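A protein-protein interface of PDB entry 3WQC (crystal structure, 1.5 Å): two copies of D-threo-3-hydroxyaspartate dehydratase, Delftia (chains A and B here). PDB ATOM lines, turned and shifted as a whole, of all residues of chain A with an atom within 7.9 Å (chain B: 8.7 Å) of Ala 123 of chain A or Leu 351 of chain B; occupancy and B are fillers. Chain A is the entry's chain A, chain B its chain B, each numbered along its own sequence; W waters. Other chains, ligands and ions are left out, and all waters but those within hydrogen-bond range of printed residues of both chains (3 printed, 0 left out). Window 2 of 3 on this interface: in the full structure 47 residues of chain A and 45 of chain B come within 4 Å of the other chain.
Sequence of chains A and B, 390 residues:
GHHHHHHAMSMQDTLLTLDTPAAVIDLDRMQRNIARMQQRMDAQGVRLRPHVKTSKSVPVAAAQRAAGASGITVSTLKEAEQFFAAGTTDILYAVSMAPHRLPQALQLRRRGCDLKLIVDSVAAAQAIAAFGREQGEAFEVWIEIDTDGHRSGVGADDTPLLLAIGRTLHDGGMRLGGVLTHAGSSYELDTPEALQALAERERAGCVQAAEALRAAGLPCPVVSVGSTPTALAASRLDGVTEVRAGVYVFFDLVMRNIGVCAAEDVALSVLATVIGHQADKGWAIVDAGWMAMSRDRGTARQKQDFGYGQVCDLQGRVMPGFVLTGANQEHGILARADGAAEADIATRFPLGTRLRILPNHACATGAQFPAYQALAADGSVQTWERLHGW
No position is printed for both chains. Of the 4 pairs that touch across the chains among the printed residues, none has its exchanged pair printed and touching as well.
OG of Ser 121 of chain A is in hydrogen-bond range of N of Ala 124 of chain A (3.1 Å). O of Ile 285 of chain B is in hydrogen-bond range of N of Ile 275 of chain B, 2.8 Å away.
Hydrophobic or aromatic side chains of chain A within 4 Å of the printed part of chain B: Ala 98, Ala 123 and Ala 124. Of the 17 printed residues of chain B, 2 touch a printed residue of chain A.
Printed residues of chain B within 4 Å of Ser 96 of chain A: Ile 275. Of the printed residues of chain B, Ala 98 of chain A touches Ile 275 (3.96 Å). Ala 123 of chain A touches just one residue of chain B: Leu 351. Printed residues of chain B within 4 Å of Ala 124 of chain A: Leu 351. Of the printed residues of chain A, Ile 275 of chain B touches Ser 96 (3.5 Å) and Ala 98 (3.96 Å). Thr 347 of chain B touches none of the printed residues of chain A. Leu 351 of chain B touches two residues of chain A. The nearest residue of chain B that does not touch Ala 123 of chain A is Pro 350 of chain B (7.7 Å). The nearest printed residue of chain B that does not touch Ala 98 of chain A is Thr 273 of chain B (4.6 Å).
Among the printed residues, pairs that only touch across the chains: Ser 96 of chain A with Ile 275 of chain B (3.5 Å), Ala 98 of chain A with Ile 275 of chain B (3.96 Å), Ala 123 of chain A with Leu 351 of chain B (3.8 Å) and Ala 124 of chain A with Leu 351 of chain B (3.5 Å).
Water W1 bridges the side-chain carboxylate of Asp 120 of chain A (2.4 Å) and the backbone carbonyl oxygen of His 277 of chain B (2.8 Å). Water W3 bridges O of Ile 275 of chain B and O of Met 97 of chain A. Water W2 bridges OD1 of Asp 120 of chain A and N of His 277 of chain B.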
ATOM      1  N   SER A  96      13.125   3.434 -26.727  1.00  0.00           N
ATOM      2  CA  SER A  96      14.081   4.413 -27.225  1.00  0.00           C
ATOM      3  C   SER A  96      14.884   3.809 -28.386  1.00  0.00           C
ATOM      4  O   SER A  96      15.553   2.780 -28.184  1.00  0.00           O
ATOM      5  CB  SER A  96      15.084   4.787 -26.144  1.00  0.00           C
ATOM      6  OG  SER A  96      14.364   5.296 -25.065  1.00  0.00           O
ATOM      7  N   MET A  97      14.937   4.492 -29.552  1.00  0.00           N
ATOM      8  CA  MET A  97      15.518   3.853 -30.731  1.00  0.00           C
ATOM      9  C   MET A  97      17.034   3.751 -30.606  1.00  0.00           C
ATOM     10  O   MET A  97      17.739   4.796 -30.312  1.00  0.00           O
ATOM     11  CB  MET A  97      15.131   4.702 -31.979  1.00  0.00           C
ATOM     12  CG  MET A  97      15.742   4.179 -33.260  1.00  0.00           C
ATOM     13  SD  MET A  97      15.052   2.507 -33.534  1.00  0.00           S
ATOM     14  CE  MET A  97      15.901   2.186 -35.154  1.00  0.00           C
ATOM     15  N   ALA A  98      17.625   2.573 -30.847  1.00  0.00           N
ATOM     16  CA  ALA A  98      19.034   2.391 -30.942  1.00  0.00           C
ATOM     17  C   ALA A  98      19.498   2.670 -32.394  1.00  0.00           C
ATOM     18  O   ALA A  98      18.954   2.134 -33.347  1.00  0.00           O
ATOM     19  CB  ALA A  98      19.351   0.923 -30.651  1.00  0.00           C
ATOM     20  N   PRO A  99      20.494   3.593 -32.548  1.00  0.00           N
ATOM     21  CA  PRO A  99      20.920   3.922 -33.946  1.00  0.00           C
ATOM     22  C   PRO A  99      21.310   2.696 -34.775  1.00  0.00           C
ATOM     23  O   PRO A  99      21.038   2.678 -35.968  1.00  0.00           O
ATOM     24  CB  PRO A  99      22.114   4.864 -33.702  1.00  0.00           C
ATOM     25  CG  PRO A  99      21.734   5.613 -32.402  1.00  0.00           C
ATOM     26  CD  PRO A  99      21.108   4.506 -31.541  1.00  0.00           C
ATOM     27  N   LEU A 102      18.676   1.315 -37.075  1.00  0.00           N
ATOM     28  CA  LEU A 102      18.073   2.139 -38.163  1.00  0.00           C
ATOM     29  C   LEU A 102      17.963   1.401 -39.526  1.00  0.00           C
ATOM     30  O   LEU A 102      16.953   1.597 -40.208  1.00  0.00           O
ATOM     31  CB  LEU A 102      18.840   3.471 -38.245  1.00  0.00           C
ATOM     32  CG  LEU A 102      18.365   4.482 -37.173  1.00  0.00           C
ATOM     33  CD1 LEU A 102      19.352   5.637 -37.029  1.00  0.00           C
ATOM     34  CD2 LEU A 102      16.951   5.028 -37.487  1.00  0.00           C
ATOM     35  N   VAL A 119      12.255   8.701 -29.361  1.00  0.00           N
ATOM     36  CA  VAL A 119      13.599   9.068 -28.820  1.00  0.00           C
ATOM     37  C   VAL A 119      13.361   9.977 -27.593  1.00  0.00           C
ATOM     38  O   VAL A 119      12.272  10.558 -27.431  1.00  0.00           O
ATOM     39  CB  VAL A 119      14.466   9.882 -29.827  1.00  0.00           C
ATOM     40  CG1 VAL A 119      14.829   9.006 -31.099  1.00  0.00           C
ATOM     41  CG2 VAL A 119      13.802  11.253 -30.195  1.00  0.00           C
ATOM     42  N   ASP A 120      14.423  10.146 -26.799  1.00  0.00           N
ATOM     43  CA  ASP A 120      14.373  11.092 -25.661  1.00  0.00           C
ATOM     44  C   ASP A 120      15.686  11.793 -25.503  1.00  0.00           C
ATOM     45  O   ASP A 120      15.954  12.393 -24.427  1.00  0.00           O
ATOM     46  CB  ASP A 120      13.947  10.387 -24.354  1.00  0.00           C
ATOM     47  CG  ASP A 120      14.974   9.387 -23.859  1.00  0.00           C
ATOM     48  OD1 ASP A 120      16.071   9.235 -24.468  1.00  0.00           O
ATOM     49  OD2 ASP A 120      14.770   8.750 -22.800  1.00  0.00           O
ATOM     50  N   SER A 121      16.530  11.811 -26.555  1.00  0.00           N
ATOM     51  CA  SER A 121      17.810  12.500 -26.464  1.00  0.00           C
ATOM     52  C   SER A 121      18.142  13.196 -27.787  1.00  0.00           C
ATOM     53  O   SER A 121      17.709  12.749 -28.882  1.00  0.00           O
ATOM     54  CB  SER A 121      18.935  11.497 -26.081  1.00  0.00           C
ATOM     55  OG  SER A 121      19.182  10.585 -27.154  1.00  0.00           O
ATOM     56  N   VAL A 122      18.916  14.276 -27.700  1.00  0.00           N
ATOM     57  CA  VAL A 122      19.442  14.918 -28.912  1.00  0.00           C
ATOM     58  C   VAL A 122      20.311  13.975 -29.718  1.00  0.00           C
ATOM     59  O   VAL A 122      20.124  13.913 -30.957  1.00  0.00           O
ATOM     60  CB  VAL A 122      20.175  16.233 -28.558  1.00  0.00           C
ATOM     61  CG1 VAL A 122      20.925  16.801 -29.783  1.00  0.00           C
ATOM     62  CG2 VAL A 122      19.195  17.271 -27.957  1.00  0.00           C
ATOM     63  N   ALA A 123      21.178  13.169 -29.080  1.00  0.00           N
ATOM     64  CA  ALA A 123      22.047  12.275 -29.878  1.00  0.00           C
ATOM     65  C   ALA A 123      21.242  11.255 -30.661  1.00  0.00           C
ATOM     66  O   ALA A 123      21.583  10.975 -31.868  1.00  0.00           O
ATOM     67  CB  ALA A 123      23.051  11.533 -28.989  1.00  0.00           C
ATOM     68  N   ALA A 124      20.187  10.680 -30.047  1.00  0.00           N
ATOM     69  CA  ALA A 124      19.406   9.673 -30.815  1.00  0.00           C
ATOM     70  C   ALA A 124      18.642  10.402 -31.979  1.00  0.00           C
ATOM     71  O   ALA A 124      18.554   9.860 -33.088  1.00  0.00           O
ATOM     72  CB  ALA A 124      18.399   8.946 -29.906  1.00  0.00           C
ATOM     73  N   ALA A 125      18.117  11.610 -31.705  1.00  0.00           N
ATOM     74  CA  ALA A 125      17.411  12.346 -32.749  1.00  0.00           C
ATOM     75  C   ALA A 125      18.351  12.713 -33.916  1.00  0.00           C
ATOM     76  O   ALA A 125      17.955  12.531 -35.120  1.00  0.00           O
ATOM     77  CB  ALA A 125      16.773  13.583 -32.161  1.00  0.00           C
ATOM     78  N   GLN A 126      19.612  13.085 -33.576  1.00  0.00           N
ATOM     79  CA  GLN A 126      20.591  13.433 -34.641  1.00  0.00           C
ATOM     80  C   GLN A 126      20.949  12.216 -35.483  1.00  0.00           C
ATOM     81  O   GLN A 126      21.117  12.313 -36.718  1.00  0.00           O
ATOM     82  CB  GLN A 126      21.848  13.996 -34.027  1.00  0.00           C
ATOM     83  CG  GLN A 126      21.678  15.365 -33.327  1.00  0.00           C
ATOM     84  CD  GLN A 126      22.954  15.848 -32.642  1.00  0.00           C
ATOM     85  OE1 GLN A 126      23.710  15.071 -32.027  1.00  0.00           O
ATOM     86  NE2 GLN A 126      23.206  17.145 -32.727  1.00  0.00           N
ATOM     87  N   ALA A 127      21.055  11.040 -34.812  1.00  0.00           N
ATOM     88  CA  ALA A 127      21.437   9.800 -35.563  1.00  0.00           C
ATOM     89  C   ALA A 127      20.288   9.469 -36.566  1.00  0.00           C
ATOM     90  O   ALA A 127      20.559   9.075 -37.730  1.00  0.00           O
ATOM     91  CB  ALA A 127      21.697   8.609 -34.629  1.00  0.00           C
ATOM     92  N   ILE A 128      19.041   9.521 -36.071  1.00  0.00           N
ATOM     93  CA  ILE A 128      17.904   9.262 -36.986  1.00  0.00           C
ATOM     94  C   ILE A 128      17.848  10.249 -38.155  1.00  0.00           C
ATOM     95  O   ILE A 128      17.786   9.830 -39.320  1.00  0.00           O
ATOM     96  CB  ILE A 128      16.551   9.250 -36.257  1.00  0.00           C
ATOM     97  CG1 ILE A 128      16.549   8.122 -35.203  1.00  0.00           C
ATOM     98  CG2 ILE A 128      15.418   9.037 -37.294  1.00  0.00           C
ATOM     99  CD1 ILE A 128      15.246   8.123 -34.322  1.00  0.00           C
ATOM    100  N   ALA A 129      17.950  11.553 -37.803  1.00  0.00           N
ATOM    101  CA  ALA A 129      17.823  12.586 -38.862  1.00  0.00           C
ATOM    102  C   ALA A 129      18.958  12.479 -39.916  1.00  0.00           C
ATOM    103  O   ALA A 129      18.674  12.499 -41.141  1.00  0.00           O
ATOM    104  CB  ALA A 129      17.768  13.963 -38.233  1.00  0.00           C
ATOM    105  N   ALA A 130      20.194  12.221 -39.459  1.00  0.00           N
ATOM    106  CA  ALA A 130      21.347  12.105 -40.361  1.00  0.00           C
ATOM    107  C   ALA A 130      21.185  10.882 -41.298  1.00  0.00           C
ATOM    108  O   ALA A 130      21.320  10.961 -42.536  1.00  0.00           O
ATOM    109  CB  ALA A 130      22.709  12.070 -39.585  1.00  0.00           C
ATOM    110  N   LEU A 161      15.372  20.662 -23.218  1.00  0.00           N
ATOM    111  CA  LEU A 161      15.708  19.383 -23.840  1.00  0.00           C
ATOM    112  C   LEU A 161      14.601  18.992 -24.879  1.00  0.00           C
ATOM    113  O   LEU A 161      14.914  18.584 -26.046  1.00  0.00           O
ATOM    114  CB  LEU A 161      15.988  18.237 -22.829  1.00  0.00           C
ATOM    115  CG  LEU A 161      16.217  16.840 -23.421  1.00  0.00           C
ATOM    116  CD1 LEU A 161      17.376  16.842 -24.394  1.00  0.00           C
ATOM    117  CD2 LEU A 161      16.468  15.827 -22.296  1.00  0.00           C
ATOM    118  N   ILE A 165      15.324  18.512 -28.973  1.00  0.00           N
ATOM    119  CA  ILE A 165      15.033  17.293 -29.727  1.00  0.00           C
ATOM    120  C   ILE A 165      14.035  17.602 -30.853  1.00  0.00           C
ATOM    121  O   ILE A 165      14.220  17.096 -32.001  1.00  0.00           O
ATOM    122  CB  ILE A 165      14.464  16.180 -28.792  1.00  0.00           C
ATOM    123  CG1 ILE A 165      15.530  15.824 -27.742  1.00  0.00           C
ATOM    124  CG2 ILE A 165      14.049  14.926 -29.628  1.00  0.00           C
ATOM    125  CD1 ILE A 165      14.939  15.029 -26.591  1.00  0.00           C
ATOM    126  N   THR A 168      15.805  19.266 -33.615  1.00  0.00           N
ATOM    127  CA  THR A 168      16.721  18.372 -34.344  1.00  0.00           C
ATOM    128  C   THR A 168      15.898  17.579 -35.392  1.00  0.00           C
ATOM    129  O   THR A 168      16.354  17.366 -36.547  1.00  0.00           O
ATOM    130  CB  THR A 168      17.422  17.419 -33.352  1.00  0.00           C
ATOM    131  OG1 THR A 168      18.212  18.209 -32.490  1.00  0.00           O
ATOM    132  CG2 THR A 168      18.373  16.415 -34.069  1.00  0.00           C
ATOM    133  N   THR B 273      22.843  -3.101 -25.678  1.00  0.00           N
ATOM    134  CA  THR B 273      23.218  -1.751 -26.100  1.00  0.00           C
ATOM    135  C   THR B 273      22.651  -0.699 -25.175  1.00  0.00           C
ATOM    136  O   THR B 273      21.448  -0.799 -24.752  1.00  0.00           O
ATOM    137  CB  THR B 273      22.638  -1.485 -27.545  1.00  0.00           C
ATOM    138  OG1 THR B 273      23.249  -2.408 -28.447  1.00  0.00           O
ATOM    139  CG2 THR B 273      22.992  -0.098 -28.070  1.00  0.00           C
ATOM    140  N   VAL B 274      23.436   0.402 -24.929  1.00  0.00           N
ATOM    141  CA  VAL B 274      22.892   1.515 -24.203  1.00  0.00           C
ATOM    142  C   VAL B 274      21.970   2.353 -25.144  1.00  0.00           C
ATOM    143  O   VAL B 274      22.402   2.758 -26.253  1.00  0.00           O
ATOM    144  CB  VAL B 274      24.058   2.415 -23.722  1.00  0.00           C
ATOM    145  CG1 VAL B 274      23.445   3.679 -23.066  1.00  0.00           C
ATOM    146  CG2 VAL B 274      24.869   1.660 -22.648  1.00  0.00           C
ATOM    147  N   ILE B 275      20.696   2.532 -24.760  1.00  0.00           N
ATOM    148  CA  ILE B 275      19.741   3.220 -25.583  1.00  0.00           C
ATOM    149  C   ILE B 275      19.241   4.544 -24.961  1.00  0.00           C
ATOM    150  O   ILE B 275      18.469   5.287 -25.588  1.00  0.00           O
ATOM    151  CB  ILE B 275      18.511   2.308 -25.900  1.00  0.00           C
ATOM    152  CG1 ILE B 275      17.824   1.862 -24.595  1.00  0.00           C
ATOM    153  CG2 ILE B 275      18.962   1.092 -26.715  1.00  0.00           C
ATOM    154  CD1 ILE B 275      16.472   1.116 -24.825  1.00  0.00           C
ATOM    155  N   GLY B 276      19.730   4.900 -23.777  1.00  0.00           N
ATOM    156  CA  GLY B 276      19.286   6.164 -23.177  1.00  0.00           C
ATOM    157  C   GLY B 276      19.866   6.336 -21.802  1.00  0.00           C
ATOM    158  O   GLY B 276      20.644   5.477 -21.346  1.00  0.00           O
ATOM    159  N   HIS B 277      19.528   7.462 -21.155  1.00  0.00           N
ATOM    160  CA  HIS B 277      19.956   7.749 -19.800  1.00  0.00           C
ATOM    161  C   HIS B 277      18.895   8.485 -18.987  1.00  0.00           C
ATOM    162  O   HIS B 277      17.997   9.148 -19.556  1.00  0.00           O
ATOM    163  CB  HIS B 277      21.193   8.661 -19.838  1.00  0.00           C
ATOM    164  CG  HIS B 277      22.352   8.086 -20.587  1.00  0.00           C
ATOM    165  ND1 HIS B 277      22.541   8.229 -21.956  1.00  0.00           N
ATOM    166  CD2 HIS B 277      23.328   7.224 -20.155  1.00  0.00           C
ATOM    167  CE1 HIS B 277      23.652   7.552 -22.331  1.00  0.00           C
ATOM    168  NE2 HIS B 277      24.125   6.914 -21.235  1.00  0.00           N
ATOM    169  N   ALA B 284      21.958   4.502 -16.751  1.00  0.00           N
ATOM    170  CA  ALA B 284      21.996   4.240 -18.206  1.00  0.00           C
ATOM    171  C   ALA B 284      20.869   3.233 -18.473  1.00  0.00           C
ATOM    172  O   ALA B 284      20.638   2.344 -17.674  1.00  0.00           O
ATOM    173  CB  ALA B 284      23.369   3.650 -18.640  1.00  0.00           C
ATOM    174  N   ILE B 285      20.146   3.389 -19.579  1.00  0.00           N
ATOM    175  CA  ILE B 285      19.081   2.464 -19.915  1.00  0.00           C
ATOM    176  C   ILE B 285      19.624   1.572 -21.041  1.00  0.00           C
ATOM    177  O   ILE B 285      20.174   2.079 -22.069  1.00  0.00           O
ATOM    178  CB  ILE B 285      17.805   3.241 -20.389  1.00  0.00           C
ATOM    179  CG1 ILE B 285      17.309   4.363 -19.406  1.00  0.00           C
ATOM    180  CG2 ILE B 285      16.726   2.233 -20.776  1.00  0.00           C
ATOM    181  CD1 ILE B 285      17.263   3.961 -18.064  1.00  0.00           C
ATOM    182  N   ILE B 345      27.058   9.813 -16.027  1.00  0.00           N
ATOM    183  CA  ILE B 345      26.700   8.442 -16.493  1.00  0.00           C
ATOM    184  C   ILE B 345      26.734   8.361 -18.030  1.00  0.00           C
ATOM    185  O   ILE B 345      27.161   7.333 -18.581  1.00  0.00           O
ATOM    186  CB  ILE B 345      25.340   7.909 -15.934  1.00  0.00           C
ATOM    187  CG1 ILE B 345      25.195   6.392 -16.220  1.00  0.00           C
ATOM    188  CG2 ILE B 345      24.156   8.697 -16.464  1.00  0.00           C
ATOM    189  CD1 ILE B 345      26.051   5.505 -15.318  1.00  0.00           C
ATOM    190  N   ALA B 346      26.337   9.459 -18.718  1.00  0.00           N
ATOM    191  CA  ALA B 346      26.372   9.475 -20.203  1.00  0.00           C
ATOM    192  C   ALA B 346      27.815   9.380 -20.786  1.00  0.00           C
ATOM    193  O   ALA B 346      28.012   8.862 -21.893  1.00  0.00           O
ATOM    194  CB  ALA B 346      25.610  10.693 -20.767  1.00  0.00           C
ATOM    195  N   THR B 347      28.814   9.925 -20.068  1.00  0.00           N
ATOM    196  CA  THR B 347      30.236   9.828 -20.511  1.00  0.00           C
ATOM    197  C   THR B 347      30.741   8.415 -20.167  1.00  0.00           C
ATOM    198  O   THR B 347      31.481   7.794 -20.939  1.00  0.00           O
ATOM    199  CB  THR B 347      31.167  11.100 -20.059  1.00  0.00           C
ATOM    200  OG1 THR B 347      31.558  10.925 -18.712  1.00  0.00           O
ATOM    201  CG2 THR B 347      30.406  12.395 -20.204  1.00  0.00           C
ATOM    202  N   ARG B 348      30.310   7.868 -19.027  1.00  0.00           N
ATOM    203  CA  ARG B 348      30.754   6.519 -18.701  1.00  0.00           C
ATOM    204  C   ARG B 348      30.185   5.442 -19.665  1.00  0.00           C
ATOM    205  O   ARG B 348      30.843   4.455 -20.010  1.00  0.00           O
ATOM    206  CB  ARG B 348      30.392   6.161 -17.281  1.00  0.00           C
ATOM    207  CG  ARG B 348      31.048   4.857 -16.921  1.00  0.00           C
ATOM    208  CD  ARG B 348      32.545   4.994 -16.960  1.00  0.00           C
ATOM    209  NE  ARG B 348      32.829   5.194 -15.560  1.00  0.00           N
ATOM    210  CZ  ARG B 348      33.167   4.227 -14.725  1.00  0.00           C
ATOM    211  NH1 ARG B 348      33.384   2.996 -15.181  1.00  0.00           N
ATOM    212  NH2 ARG B 348      33.378   4.538 -13.454  1.00  0.00           N
ATOM    213  N   PHE B 349      28.936   5.631 -20.016  1.00  0.00           N
ATOM    214  CA  PHE B 349      28.181   4.705 -20.867  1.00  0.00           C
ATOM    215  C   PHE B 349      27.505   5.447 -22.034  1.00  0.00           C
ATOM    216  O   PHE B 349      26.290   5.627 -22.026  1.00  0.00           O
ATOM    217  CB  PHE B 349      27.156   3.913 -20.023  1.00  0.00           C
ATOM    218  CG  PHE B 349      27.785   3.044 -18.987  1.00  0.00           C
ATOM    219  CD1 PHE B 349      28.371   1.783 -19.352  1.00  0.00           C
ATOM    220  CD2 PHE B 349      27.812   3.427 -17.631  1.00  0.00           C
ATOM    221  CE1 PHE B 349      28.961   0.966 -18.334  1.00  0.00           C
ATOM    222  CE2 PHE B 349      28.419   2.625 -16.664  1.00  0.00           C
ATOM    223  CZ  PHE B 349      28.996   1.411 -17.003  1.00  0.00           C
ATOM    224  N   PRO B 350      28.257   5.783 -23.103  1.00  0.00           N
ATOM    225  CA  PRO B 350      27.588   6.633 -24.157  1.00  0.00           C
ATOM    226  C   PRO B 350      26.481   5.880 -24.950  1.00  0.00           C
ATOM    227  O   PRO B 350      26.526   4.606 -25.060  1.00  0.00           O
ATOM    228  CB  PRO B 350      28.764   6.997 -25.105  1.00  0.00           C
ATOM    229  CG  PRO B 350      29.957   6.802 -24.247  1.00  0.00           C
ATOM    230  CD  PRO B 350      29.715   5.698 -23.293  1.00  0.00           C
ATOM    231  N   LEU B 351      25.477   6.601 -25.460  1.00  0.00           N
ATOM    232  CA  LEU B 351      24.483   6.008 -26.308  1.00  0.00           C
ATOM    233  C   LEU B 351      25.146   5.140 -27.362  1.00  0.00           C
ATOM    234  O   LEU B 351      26.196   5.538 -27.935  1.00  0.00           O
ATOM    235  CB  LEU B 351      23.628   7.127 -26.987  1.00  0.00           C
ATOM    236  CG  LEU B 351      22.536   6.746 -28.047  1.00  0.00           C
ATOM    237  CD1 LEU B 351      21.346   6.059 -27.396  1.00  0.00           C
ATOM    238  CD2 LEU B 351      22.012   7.906 -28.948  1.00  0.00           C
ATOM    239  N   GLY B 352      24.606   3.919 -27.549  1.00  0.00           N
ATOM    240  CA  GLY B 352      25.156   2.973 -28.513  1.00  0.00           C
ATOM    241  C   GLY B 352      26.298   2.102 -28.041  1.00  0.00           C
ATOM    242  O   GLY B 352      26.615   1.152 -28.730  1.00  0.00           O
ATOM    243  N   THR B 353      26.819   2.337 -26.817  1.00  0.00           N
ATOM    244  CA  THR B 353      27.845   1.446 -26.169  1.00  0.00           C
ATOM    245  C   THR B 353      27.277   0.042 -26.008  1.00  0.00           C
ATOM    246  O   THR B 353      26.088  -0.101 -25.610  1.00  0.00           O
ATOM    247  CB  THR B 353      28.203   1.953 -24.748  1.00  0.00           C
ATOM    248  OG1 THR B 353      28.691   3.259 -24.852  1.00  0.00           O
ATOM    249  CG2 THR B 353      29.266   1.071 -24.029  1.00  0.00           C
ATOM    250  N   ARG B 354      28.087  -0.928 -26.384  1.00  0.00           N
ATOM    251  CA  ARG B 354      27.721  -2.357 -26.153  1.00  0.00           C
ATOM    252  C   ARG B 354      28.361  -2.854 -24.879  1.00  0.00           C
ATOM    253  O   ARG B 354      29.585  -2.607 -24.612  1.00  0.00           O
ATOM    254  CB  ARG B 354      28.184  -3.222 -27.309  1.00  0.00           C
ATOM    255  CG  ARG B 354      27.359  -2.939 -28.521  1.00  0.00           C
ATOM    256  CD  ARG B 354      27.741  -3.746 -29.704  1.00  0.00           C
ATOM    257  NE  ARG B 354      26.641  -3.417 -30.629  1.00  0.00           N
ATOM    258  CZ  ARG B 354      25.953  -4.273 -31.372  1.00  0.00           C
ATOM    259  NH1 ARG B 354      26.353  -5.517 -31.477  1.00  0.00           N
ATOM    260  NH2 ARG B 354      24.920  -3.817 -32.084  1.00  0.00           N
HETATM  261  O   HOH W   1      16.113   7.736 -21.065  1.00  0.00           O
HETATM  262  O   HOH W   2      18.409   9.509 -22.975  1.00  0.00           O
HETATM  263  O   HOH W   3      17.740   6.244 -27.976  1.00  0.00           O
